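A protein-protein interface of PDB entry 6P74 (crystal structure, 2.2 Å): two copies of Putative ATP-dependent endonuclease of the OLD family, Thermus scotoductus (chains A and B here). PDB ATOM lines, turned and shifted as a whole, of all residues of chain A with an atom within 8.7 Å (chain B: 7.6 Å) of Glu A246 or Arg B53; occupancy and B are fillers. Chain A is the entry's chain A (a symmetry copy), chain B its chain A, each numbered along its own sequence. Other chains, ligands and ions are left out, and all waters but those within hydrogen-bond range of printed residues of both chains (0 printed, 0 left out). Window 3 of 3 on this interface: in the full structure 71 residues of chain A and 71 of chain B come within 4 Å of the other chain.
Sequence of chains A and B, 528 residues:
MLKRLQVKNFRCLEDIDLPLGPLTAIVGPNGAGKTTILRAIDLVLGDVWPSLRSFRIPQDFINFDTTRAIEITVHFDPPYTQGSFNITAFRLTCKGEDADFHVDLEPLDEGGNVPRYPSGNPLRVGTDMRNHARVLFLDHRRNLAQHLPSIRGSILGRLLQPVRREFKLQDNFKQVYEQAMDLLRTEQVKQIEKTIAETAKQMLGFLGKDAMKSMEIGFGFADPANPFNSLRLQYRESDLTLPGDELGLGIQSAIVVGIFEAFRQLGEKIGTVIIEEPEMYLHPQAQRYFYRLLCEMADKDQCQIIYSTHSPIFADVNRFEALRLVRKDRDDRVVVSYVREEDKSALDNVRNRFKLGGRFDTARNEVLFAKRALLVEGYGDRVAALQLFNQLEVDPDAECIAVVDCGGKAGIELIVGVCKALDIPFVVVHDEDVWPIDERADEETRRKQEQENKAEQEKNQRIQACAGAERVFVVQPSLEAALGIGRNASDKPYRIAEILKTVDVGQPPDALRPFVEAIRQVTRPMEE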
ATOM      1  N   HIS A 140       7.167  22.023   7.175  1.00  0.00           N
ATOM      2  CA  HIS A 140       5.911  21.793   7.879  1.00  0.00           C
ATOM      3  C   HIS A 140       6.153  22.668   9.102  1.00  0.00           C
ATOM      4  O   HIS A 140       6.840  22.306  10.059  1.00  0.00           O
ATOM      5  CB  HIS A 140       5.633  20.316   8.038  1.00  0.00           C
ATOM      6  CG  HIS A 140       4.810  19.779   6.917  1.00  0.00           C
ATOM      7  ND1 HIS A 140       5.372  19.298   5.754  1.00  0.00           N
ATOM      8  CD2 HIS A 140       3.468  19.734   6.735  1.00  0.00           C
ATOM      9  CE1 HIS A 140       4.411  18.931   4.925  1.00  0.00           C
ATOM     10  NE2 HIS A 140       3.247  19.189   5.496  1.00  0.00           N
ATOM     11  N   TYR A 235      -7.082  33.483  13.720  1.00  0.00           N
ATOM     12  CA  TYR A 235      -8.479  33.089  13.596  1.00  0.00           C
ATOM     13  C   TYR A 235      -8.951  32.571  14.951  1.00  0.00           C
ATOM     14  O   TYR A 235      -8.147  32.304  15.848  1.00  0.00           O
ATOM     15  CB  TYR A 235      -8.653  32.039  12.498  1.00  0.00           C
ATOM     16  CG  TYR A 235      -7.793  30.825  12.719  1.00  0.00           C
ATOM     17  CD1 TYR A 235      -6.435  30.849  12.419  1.00  0.00           C
ATOM     18  CD2 TYR A 235      -8.330  29.659  13.245  1.00  0.00           C
ATOM     19  CE1 TYR A 235      -5.637  29.736  12.633  1.00  0.00           C
ATOM     20  CE2 TYR A 235      -7.543  28.544  13.461  1.00  0.00           C
ATOM     21  CZ  TYR A 235      -6.195  28.590  13.157  1.00  0.00           C
ATOM     22  OH  TYR A 235      -5.409  27.480  13.379  1.00  0.00           O
ATOM     23  N   ASP A 245      -4.668  19.610  16.291  1.00  0.00           N
ATOM     24  CA  ASP A 245      -5.957  19.906  15.680  1.00  0.00           C
ATOM     25  C   ASP A 245      -5.866  19.761  14.177  1.00  0.00           C
ATOM     26  O   ASP A 245      -5.322  20.638  13.510  1.00  0.00           O
ATOM     27  CB  ASP A 245      -6.418  21.319  16.041  1.00  0.00           C
ATOM     28  N   GLU A 246      -6.395  18.660  13.634  1.00  0.00           N
ATOM     29  CA  GLU A 246      -6.381  18.501  12.185  1.00  0.00           C
ATOM     30  C   GLU A 246      -7.160  19.615  11.498  1.00  0.00           C
ATOM     31  O   GLU A 246      -6.784  20.052  10.406  1.00  0.00           O
ATOM     32  CB  GLU A 246      -6.939  17.134  11.784  1.00  0.00           C
ATOM     33  CG  GLU A 246      -6.444  16.661  10.408  1.00  0.00           C
ATOM     34  CD  GLU A 246      -7.188  15.444   9.879  1.00  0.00           C
ATOM     35  OE1 GLU A 246      -8.355  15.586   9.443  1.00  0.00           O
ATOM     36  OE2 GLU A 246      -6.600  14.343   9.898  1.00  0.00           O
ATOM     37  N   LEU A 247      -8.242  20.090  12.121  1.00  0.00           N
ATOM     38  CA  LEU A 247      -8.964  21.237  11.582  1.00  0.00           C
ATOM     39  C   LEU A 247      -8.073  22.472  11.569  1.00  0.00           C
ATOM     40  O   LEU A 247      -8.007  23.197  10.567  1.00  0.00           O
ATOM     41  CB  LEU A 247     -10.234  21.492  12.399  1.00  0.00           C
ATOM     42  CG  LEU A 247     -11.143  22.648  11.962  1.00  0.00           C
ATOM     43  CD1 LEU A 247     -11.858  22.318  10.656  1.00  0.00           C
ATOM     44  CD2 LEU A 247     -12.141  23.027  13.057  1.00  0.00           C
ATOM     45  N   GLY A 248      -7.369  22.719  12.675  1.00  0.00           N
ATOM     46  CA  GLY A 248      -6.443  23.837  12.718  1.00  0.00           C
ATOM     47  C   GLY A 248      -5.362  23.738  11.658  1.00  0.00           C
ATOM     48  O   GLY A 248      -4.992  24.737  11.036  1.00  0.00           O
ATOM     49  N   LEU A 249      -4.846  22.530  11.428  1.00  0.00           N
ATOM     50  CA  LEU A 249      -3.796  22.372  10.428  1.00  0.00           C
ATOM     51  C   LEU A 249      -4.312  22.701   9.034  1.00  0.00           C
ATOM     52  O   LEU A 249      -3.622  23.367   8.250  1.00  0.00           O
ATOM     53  CB  LEU A 249      -3.241  20.952  10.475  1.00  0.00           C
ATOM     54  CG  LEU A 249      -2.424  20.618  11.726  1.00  0.00           C
ATOM     55  CD1 LEU A 249      -2.217  19.104  11.842  1.00  0.00           C
ATOM     56  CD2 LEU A 249      -1.084  21.365  11.735  1.00  0.00           C
ATOM     57  N   GLY A 250      -5.524  22.231   8.705  1.00  0.00           N
ATOM     58  CA  GLY A 250      -6.115  22.565   7.420  1.00  0.00           C
ATOM     59  C   GLY A 250      -6.335  24.057   7.250  1.00  0.00           C
ATOM     60  O   GLY A 250      -6.113  24.609   6.168  1.00  0.00           O
ATOM     61  N   ILE A 251      -6.773  24.731   8.314  1.00  0.00           N
ATOM     62  CA  ILE A 251      -6.969  26.175   8.251  1.00  0.00           C
ATOM     63  C   ILE A 251      -5.648  26.873   7.960  1.00  0.00           C
ATOM     64  O   ILE A 251      -5.584  27.800   7.145  1.00  0.00           O
ATOM     65  CB  ILE A 251      -7.600  26.680   9.560  1.00  0.00           C
ATOM     66  CG1 ILE A 251      -9.043  26.196   9.681  1.00  0.00           C
ATOM     67  CG2 ILE A 251      -7.526  28.207   9.654  1.00  0.00           C
ATOM     68  CD1 ILE A 251      -9.687  26.641  10.966  1.00  0.00           C
ATOM     69  N   GLN A 252      -4.572  26.441   8.620  1.00  0.00           N
ATOM     70  CA  GLN A 252      -3.285  27.090   8.407  1.00  0.00           C
ATOM     71  C   GLN A 252      -2.753  26.837   7.010  1.00  0.00           C
ATOM     72  O   GLN A 252      -2.073  27.705   6.444  1.00  0.00           O
ATOM     73  CB  GLN A 252      -2.280  26.627   9.457  1.00  0.00           C
ATOM     74  CG  GLN A 252      -2.402  27.400  10.753  1.00  0.00           C
ATOM     75  CD  GLN A 252      -1.668  26.740  11.902  1.00  0.00           C
ATOM     76  OE1 GLN A 252      -1.119  25.644  11.755  1.00  0.00           O
ATOM     77  NE2 GLN A 252      -1.654  27.406  13.061  1.00  0.00           N
ATOM     78  N   SER A 253      -3.036  25.657   6.444  1.00  0.00           N
ATOM     79  CA  SER A 253      -2.685  25.387   5.052  1.00  0.00           C
ATOM     80  C   SER A 253      -3.484  26.271   4.109  1.00  0.00           C
ATOM     81  O   SER A 253      -2.956  26.749   3.098  1.00  0.00           O
ATOM     82  CB  SER A 253      -2.940  23.922   4.713  1.00  0.00           C
ATOM     83  OG  SER A 253      -2.011  23.106   5.367  1.00  0.00           O
ATOM     84  N   MET A 280       0.042  19.502   1.819  1.00  0.00           N
ATOM     85  CA  MET A 280      -0.384  18.897   3.071  1.00  0.00           C
ATOM     86  C   MET A 280      -1.530  19.672   3.698  1.00  0.00           C
ATOM     87  O   MET A 280      -1.516  20.908   3.761  1.00  0.00           O
ATOM     88  CB  MET A 280       0.773  18.734   4.048  1.00  0.00           C
ATOM     89  CG  MET A 280       0.670  17.339   4.685  1.00  0.00           C
ATOM     90  SD  MET A 280       2.051  16.626   5.595  1.00  0.00           S
ATOM     91  CE  MET A 280       1.688  14.873   5.492  1.00  0.00           C
ATOM     92  N   TYR A 281      -2.545  18.917   4.111  1.00  0.00           N
ATOM     93  CA  TYR A 281      -3.759  19.383   4.767  1.00  0.00           C
ATOM     94  C   TYR A 281      -4.618  20.247   3.866  1.00  0.00           C
ATOM     95  O   TYR A 281      -5.440  21.015   4.356  1.00  0.00           O
ATOM     96  CB  TYR A 281      -3.436  20.115   6.075  1.00  0.00           C
ATOM     97  CG  TYR A 281      -2.493  19.321   6.947  1.00  0.00           C
ATOM     98  CD1 TYR A 281      -2.783  18.007   7.296  1.00  0.00           C
ATOM     99  CD2 TYR A 281      -1.283  19.869   7.382  1.00  0.00           C
ATOM    100  CE1 TYR A 281      -1.905  17.262   8.080  1.00  0.00           C
ATOM    101  CE2 TYR A 281      -0.400  19.139   8.158  1.00  0.00           C
ATOM    102  CZ  TYR A 281      -0.716  17.835   8.502  1.00  0.00           C
ATOM    103  OH  TYR A 281       0.159  17.105   9.273  1.00  0.00           O
ATOM    104  N   LEU A 282      -4.468  20.128   2.549  1.00  0.00           N
ATOM    105  CA  LEU A 282      -5.373  20.769   1.601  1.00  0.00           C
ATOM    106  C   LEU A 282      -6.289  19.730   0.982  1.00  0.00           C
ATOM    107  O   LEU A 282      -5.847  18.627   0.647  1.00  0.00           O
ATOM    108  CB  LEU A 282      -4.622  21.485   0.475  1.00  0.00           C
ATOM    109  CG  LEU A 282      -3.856  22.701   0.932  1.00  0.00           C
ATOM    110  CD1 LEU A 282      -2.962  23.201  -0.199  1.00  0.00           C
ATOM    111  CD2 LEU A 282      -4.846  23.777   1.435  1.00  0.00           C
ATOM    112  N   LEU B  43       7.846  12.893  22.243  1.00  0.00           N
ATOM    113  CA  LEU B  43       6.836  12.277  21.388  1.00  0.00           C
ATOM    114  C   LEU B  43       5.597  11.916  22.184  1.00  0.00           C
ATOM    115  O   LEU B  43       4.468  12.101  21.714  1.00  0.00           O
ATOM    116  CB  LEU B  43       7.404  11.015  20.741  1.00  0.00           C
ATOM    117  CG  LEU B  43       7.922  11.160  19.327  1.00  0.00           C
ATOM    118  CD1 LEU B  43       8.442   9.833  18.810  1.00  0.00           C
ATOM    119  CD2 LEU B  43       6.772  11.648  18.508  1.00  0.00           C
ATOM    120  N   VAL B  48       2.219  18.085  21.236  1.00  0.00           N
ATOM    121  CA  VAL B  48       1.519  17.595  20.053  1.00  0.00           C
ATOM    122  C   VAL B  48       0.996  16.192  20.339  1.00  0.00           C
ATOM    123  O   VAL B  48       1.768  15.301  20.714  1.00  0.00           O
ATOM    124  CB  VAL B  48       2.426  17.591  18.810  1.00  0.00           C
ATOM    125  CG1 VAL B  48       2.084  16.406  17.901  1.00  0.00           C
ATOM    126  CG2 VAL B  48       2.256  18.884  18.057  1.00  0.00           C
ATOM    127  N   TRP B  49      -0.305  15.993  20.136  1.00  0.00           N
ATOM    128  CA  TRP B  49      -0.898  14.694  20.411  1.00  0.00           C
ATOM    129  C   TRP B  49      -0.231  13.622  19.552  1.00  0.00           C
ATOM    130  O   TRP B  49      -0.176  13.764  18.322  1.00  0.00           O
ATOM    131  CB  TRP B  49      -2.401  14.699  20.152  1.00  0.00           C
ATOM    132  CG  TRP B  49      -2.998  13.408  20.593  1.00  0.00           C
ATOM    133  CD1 TRP B  49      -3.157  12.277  19.844  1.00  0.00           C
ATOM    134  CD2 TRP B  49      -3.458  13.085  21.911  1.00  0.00           C
ATOM    135  NE1 TRP B  49      -3.712  11.279  20.608  1.00  0.00           N
ATOM    136  CE2 TRP B  49      -3.908  11.749  21.880  1.00  0.00           C
ATOM    137  CE3 TRP B  49      -3.550  13.803  23.111  1.00  0.00           C
ATOM    138  CZ2 TRP B  49      -4.439  11.115  23.000  1.00  0.00           C
ATOM    139  CZ3 TRP B  49      -4.084  13.176  24.221  1.00  0.00           C
ATOM    140  CH2 TRP B  49      -4.521  11.845  24.160  1.00  0.00           C
ATOM    141  N   PRO B  50       0.275  12.546  20.151  1.00  0.00           N
ATOM    142  CA  PRO B  50       0.967  11.503  19.375  1.00  0.00           C
ATOM    143  C   PRO B  50       0.020  10.836  18.396  1.00  0.00           C
ATOM    144  O   PRO B  50      -1.000  10.270  18.785  1.00  0.00           O
ATOM    145  CB  PRO B  50       1.433  10.508  20.446  1.00  0.00           C
ATOM    146  CG  PRO B  50       1.264  11.195  21.740  1.00  0.00           C
ATOM    147  CD  PRO B  50       0.200  12.219  21.580  1.00  0.00           C
ATOM    148  N   SER B  51       0.371  10.888  17.120  1.00  0.00           N
ATOM    149  CA  SER B  51      -0.405  10.187  16.112  1.00  0.00           C
ATOM    150  C   SER B  51       0.547   9.756  15.002  1.00  0.00           C
ATOM    151  O   SER B  51       1.768   9.908  15.112  1.00  0.00           O
ATOM    152  CB  SER B  51      -1.557  11.064  15.611  1.00  0.00           C
ATOM    153  OG  SER B  51      -1.081  12.277  15.065  1.00  0.00           O
ATOM    154  N   LEU B  52      -0.019   9.195  13.934  1.00  0.00           N
ATOM    155  CA  LEU B  52       0.801   8.778  12.807  1.00  0.00           C
ATOM    156  C   LEU B  52       1.575   9.957  12.221  1.00  0.00           C
ATOM    157  O   LEU B  52       2.666   9.771  11.670  1.00  0.00           O
ATOM    158  CB  LEU B  52      -0.087   8.108  11.754  1.00  0.00           C
ATOM    159  CG  LEU B  52       0.604   7.283  10.667  1.00  0.00           C
ATOM    160  CD1 LEU B  52       1.533   6.225  11.268  1.00  0.00           C
ATOM    161  CD2 LEU B  52      -0.443   6.641   9.743  1.00  0.00           C
ATOM    162  N   ARG B  53       1.031  11.179  12.339  1.00  0.00           N
ATOM    163  CA  ARG B  53       1.719  12.398  11.918  1.00  0.00           C
ATOM    164  C   ARG B  53       2.919  12.735  12.788  1.00  0.00           C
ATOM    165  O   ARG B  53       3.642  13.688  12.470  1.00  0.00           O
ATOM    166  CB  ARG B  53       0.766  13.596  11.940  1.00  0.00           C
ATOM    167  CG  ARG B  53      -0.251  13.656  10.819  1.00  0.00           C
ATOM    168  CD  ARG B  53      -1.224  14.815  11.038  1.00  0.00           C
ATOM    169  NE  ARG B  53      -1.645  14.900  12.436  1.00  0.00           N
ATOM    170  CZ  ARG B  53      -2.886  15.171  12.833  1.00  0.00           C
ATOM    171  NH1 ARG B  53      -3.843  15.377  11.937  1.00  0.00           N
ATOM    172  NH2 ARG B  53      -3.171  15.223  14.129  1.00  0.00           N
ATOM    173  N   SER B  54       3.135  12.009  13.884  1.00  0.00           N
ATOM    174  CA  SER B  54       4.269  12.300  14.751  1.00  0.00           C
ATOM    175  C   SER B  54       5.549  11.617  14.292  1.00  0.00           C
ATOM    176  O   SER B  54       6.641  12.062  14.664  1.00  0.00           O
ATOM    177  CB  SER B  54       3.954  11.874  16.188  1.00  0.00           C
ATOM    178  OG  SER B  54       2.796  12.522  16.680  1.00  0.00           O
ATOM    179  N   PHE B  55       5.443  10.553  13.504  1.00  0.00           N
ATOM    180  CA  PHE B  55       6.587   9.746  13.117  1.00  0.00           C
ATOM    181  C   PHE B  55       6.986  10.020  11.673  1.00  0.00           C
ATOM    182  O   PHE B  55       6.160  10.405  10.841  1.00  0.00           O
ATOM    183  CB  PHE B  55       6.282   8.254  13.284  1.00  0.00           C
ATOM    184  CG  PHE B  55       6.156   7.813  14.715  1.00  0.00           C
ATOM    185  CD1 PHE B  55       4.946   7.919  15.387  1.00  0.00           C
ATOM    186  CD2 PHE B  55       7.246   7.278  15.386  1.00  0.00           C
ATOM    187  CE1 PHE B  55       4.828   7.499  16.712  1.00  0.00           C
ATOM    188  CE2 PHE B  55       7.141   6.860  16.703  1.00  0.00           C
ATOM    189  CZ  PHE B  55       5.931   6.970  17.371  1.00  0.00           C
ATOM    190  N   ARG B  56       8.268   9.817  11.389  1.00  0.00           N
ATOM    191  CA  ARG B  56       8.766   9.700  10.026  1.00  0.00           C
ATOM    192  C   ARG B  56       8.921   8.212   9.705  1.00  0.00           C
ATOM    193  O   ARG B  56       9.599   7.479  10.439  1.00  0.00           O
ATOM    194  CB  ARG B  56      10.091  10.458   9.864  1.00  0.00           C
ATOM    195  CG  ARG B  56      10.041  11.919  10.328  1.00  0.00           C
ATOM    196  CD  ARG B  56      11.327  12.688  10.004  1.00  0.00           C
ATOM    197  NE  ARG B  56      11.118  13.686   8.947  1.00  0.00           N
ATOM    198  CZ  ARG B  56      12.031  14.575   8.546  1.00  0.00           C
ATOM    199  NH1 ARG B  56      13.235  14.606   9.114  1.00  0.00           N
ATOM    200  NH2 ARG B  56      11.739  15.440   7.577  1.00  0.00           N
ATOM    201  N   ILE B  57       8.268   7.762   8.642  1.00  0.00           N
ATOM    202  CA  ILE B  57       8.313   6.370   8.200  1.00  0.00           C
ATOM    203  C   ILE B  57       9.029   6.336   6.855  1.00  0.00           C
ATOM    204  O   ILE B  57       8.508   6.885   5.874  1.00  0.00           O
ATOM    205  CB  ILE B  57       6.911   5.750   8.084  1.00  0.00           C
ATOM    206  CG1 ILE B  57       6.225   5.705   9.445  1.00  0.00           C
ATOM    207  CG2 ILE B  57       6.990   4.354   7.496  1.00  0.00           C
ATOM    208  CD1 ILE B  57       5.677   7.034   9.885  1.00  0.00           C
ATOM    209  N   VAL B 103      -0.455   4.152  15.130  1.00  0.00           N
ATOM    210  CA  VAL B 103       0.138   4.342  16.442  1.00  0.00           C
ATOM    211  C   VAL B 103      -0.960   4.230  17.484  1.00  0.00           C
ATOM    212  O   VAL B 103      -2.101   4.641  17.246  1.00  0.00           O
ATOM    213  CB  VAL B 103       0.892   5.687  16.550  1.00  0.00           C
ATOM    214  CG1 VAL B 103       1.657   5.970  15.265  1.00  0.00           C
ATOM    215  CG2 VAL B 103      -0.055   6.814  16.866  1.00  0.00           C
ATOM    216  N   LEU B 207     -13.836  21.449   1.570  1.00  0.00           N
ATOM    217  CA  LEU B 207     -14.044  20.389   2.549  1.00  0.00           C
ATOM    218  C   LEU B 207     -15.518  20.086   2.798  1.00  0.00           C
ATOM    219  O   LEU B 207     -15.819  19.078   3.450  1.00  0.00           O
ATOM    220  CB  LEU B 207     -13.349  20.762   3.852  1.00  0.00           C
ATOM    221  CG  LEU B 207     -11.826  20.824   3.722  1.00  0.00           C
ATOM    222  CD1 LEU B 207     -11.204  21.397   4.993  1.00  0.00           C
ATOM    223  CD2 LEU B 207     -11.250  19.435   3.401  1.00  0.00           C
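The guanidinium group of Arg B53 is in salt-bridge range of the side-chain carboxylate of Glu A246 (3.6 Å).
Among the printed residues, merely in contact across the chains: Tyr A281 with Arg B53.
Glu A246 touches one residue of chain B.
Of the printed residues of chain B, Tyr A281 touches Arg B53.
Val B48 touches none of the printed residues of chain A.
Ser B51 touches none of the printed residues of chain A.
Arg B53 touches two residues of chain A.
No residue of chain A comes within 4 Å of Ser B54.
The nearest residue of chain A that does not touch Arg B53 is Leu A249 (4.1 Å).
Among the printed residues, 2 pairs touch across the chains.
Among the printed residues, Asp or Glu carboxylates within 4 Å of a Lys or Arg side-chain nitrogen of the other chain: Glu A246 with Arg B53 (3.6 Å).
No position is printed for both chains.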
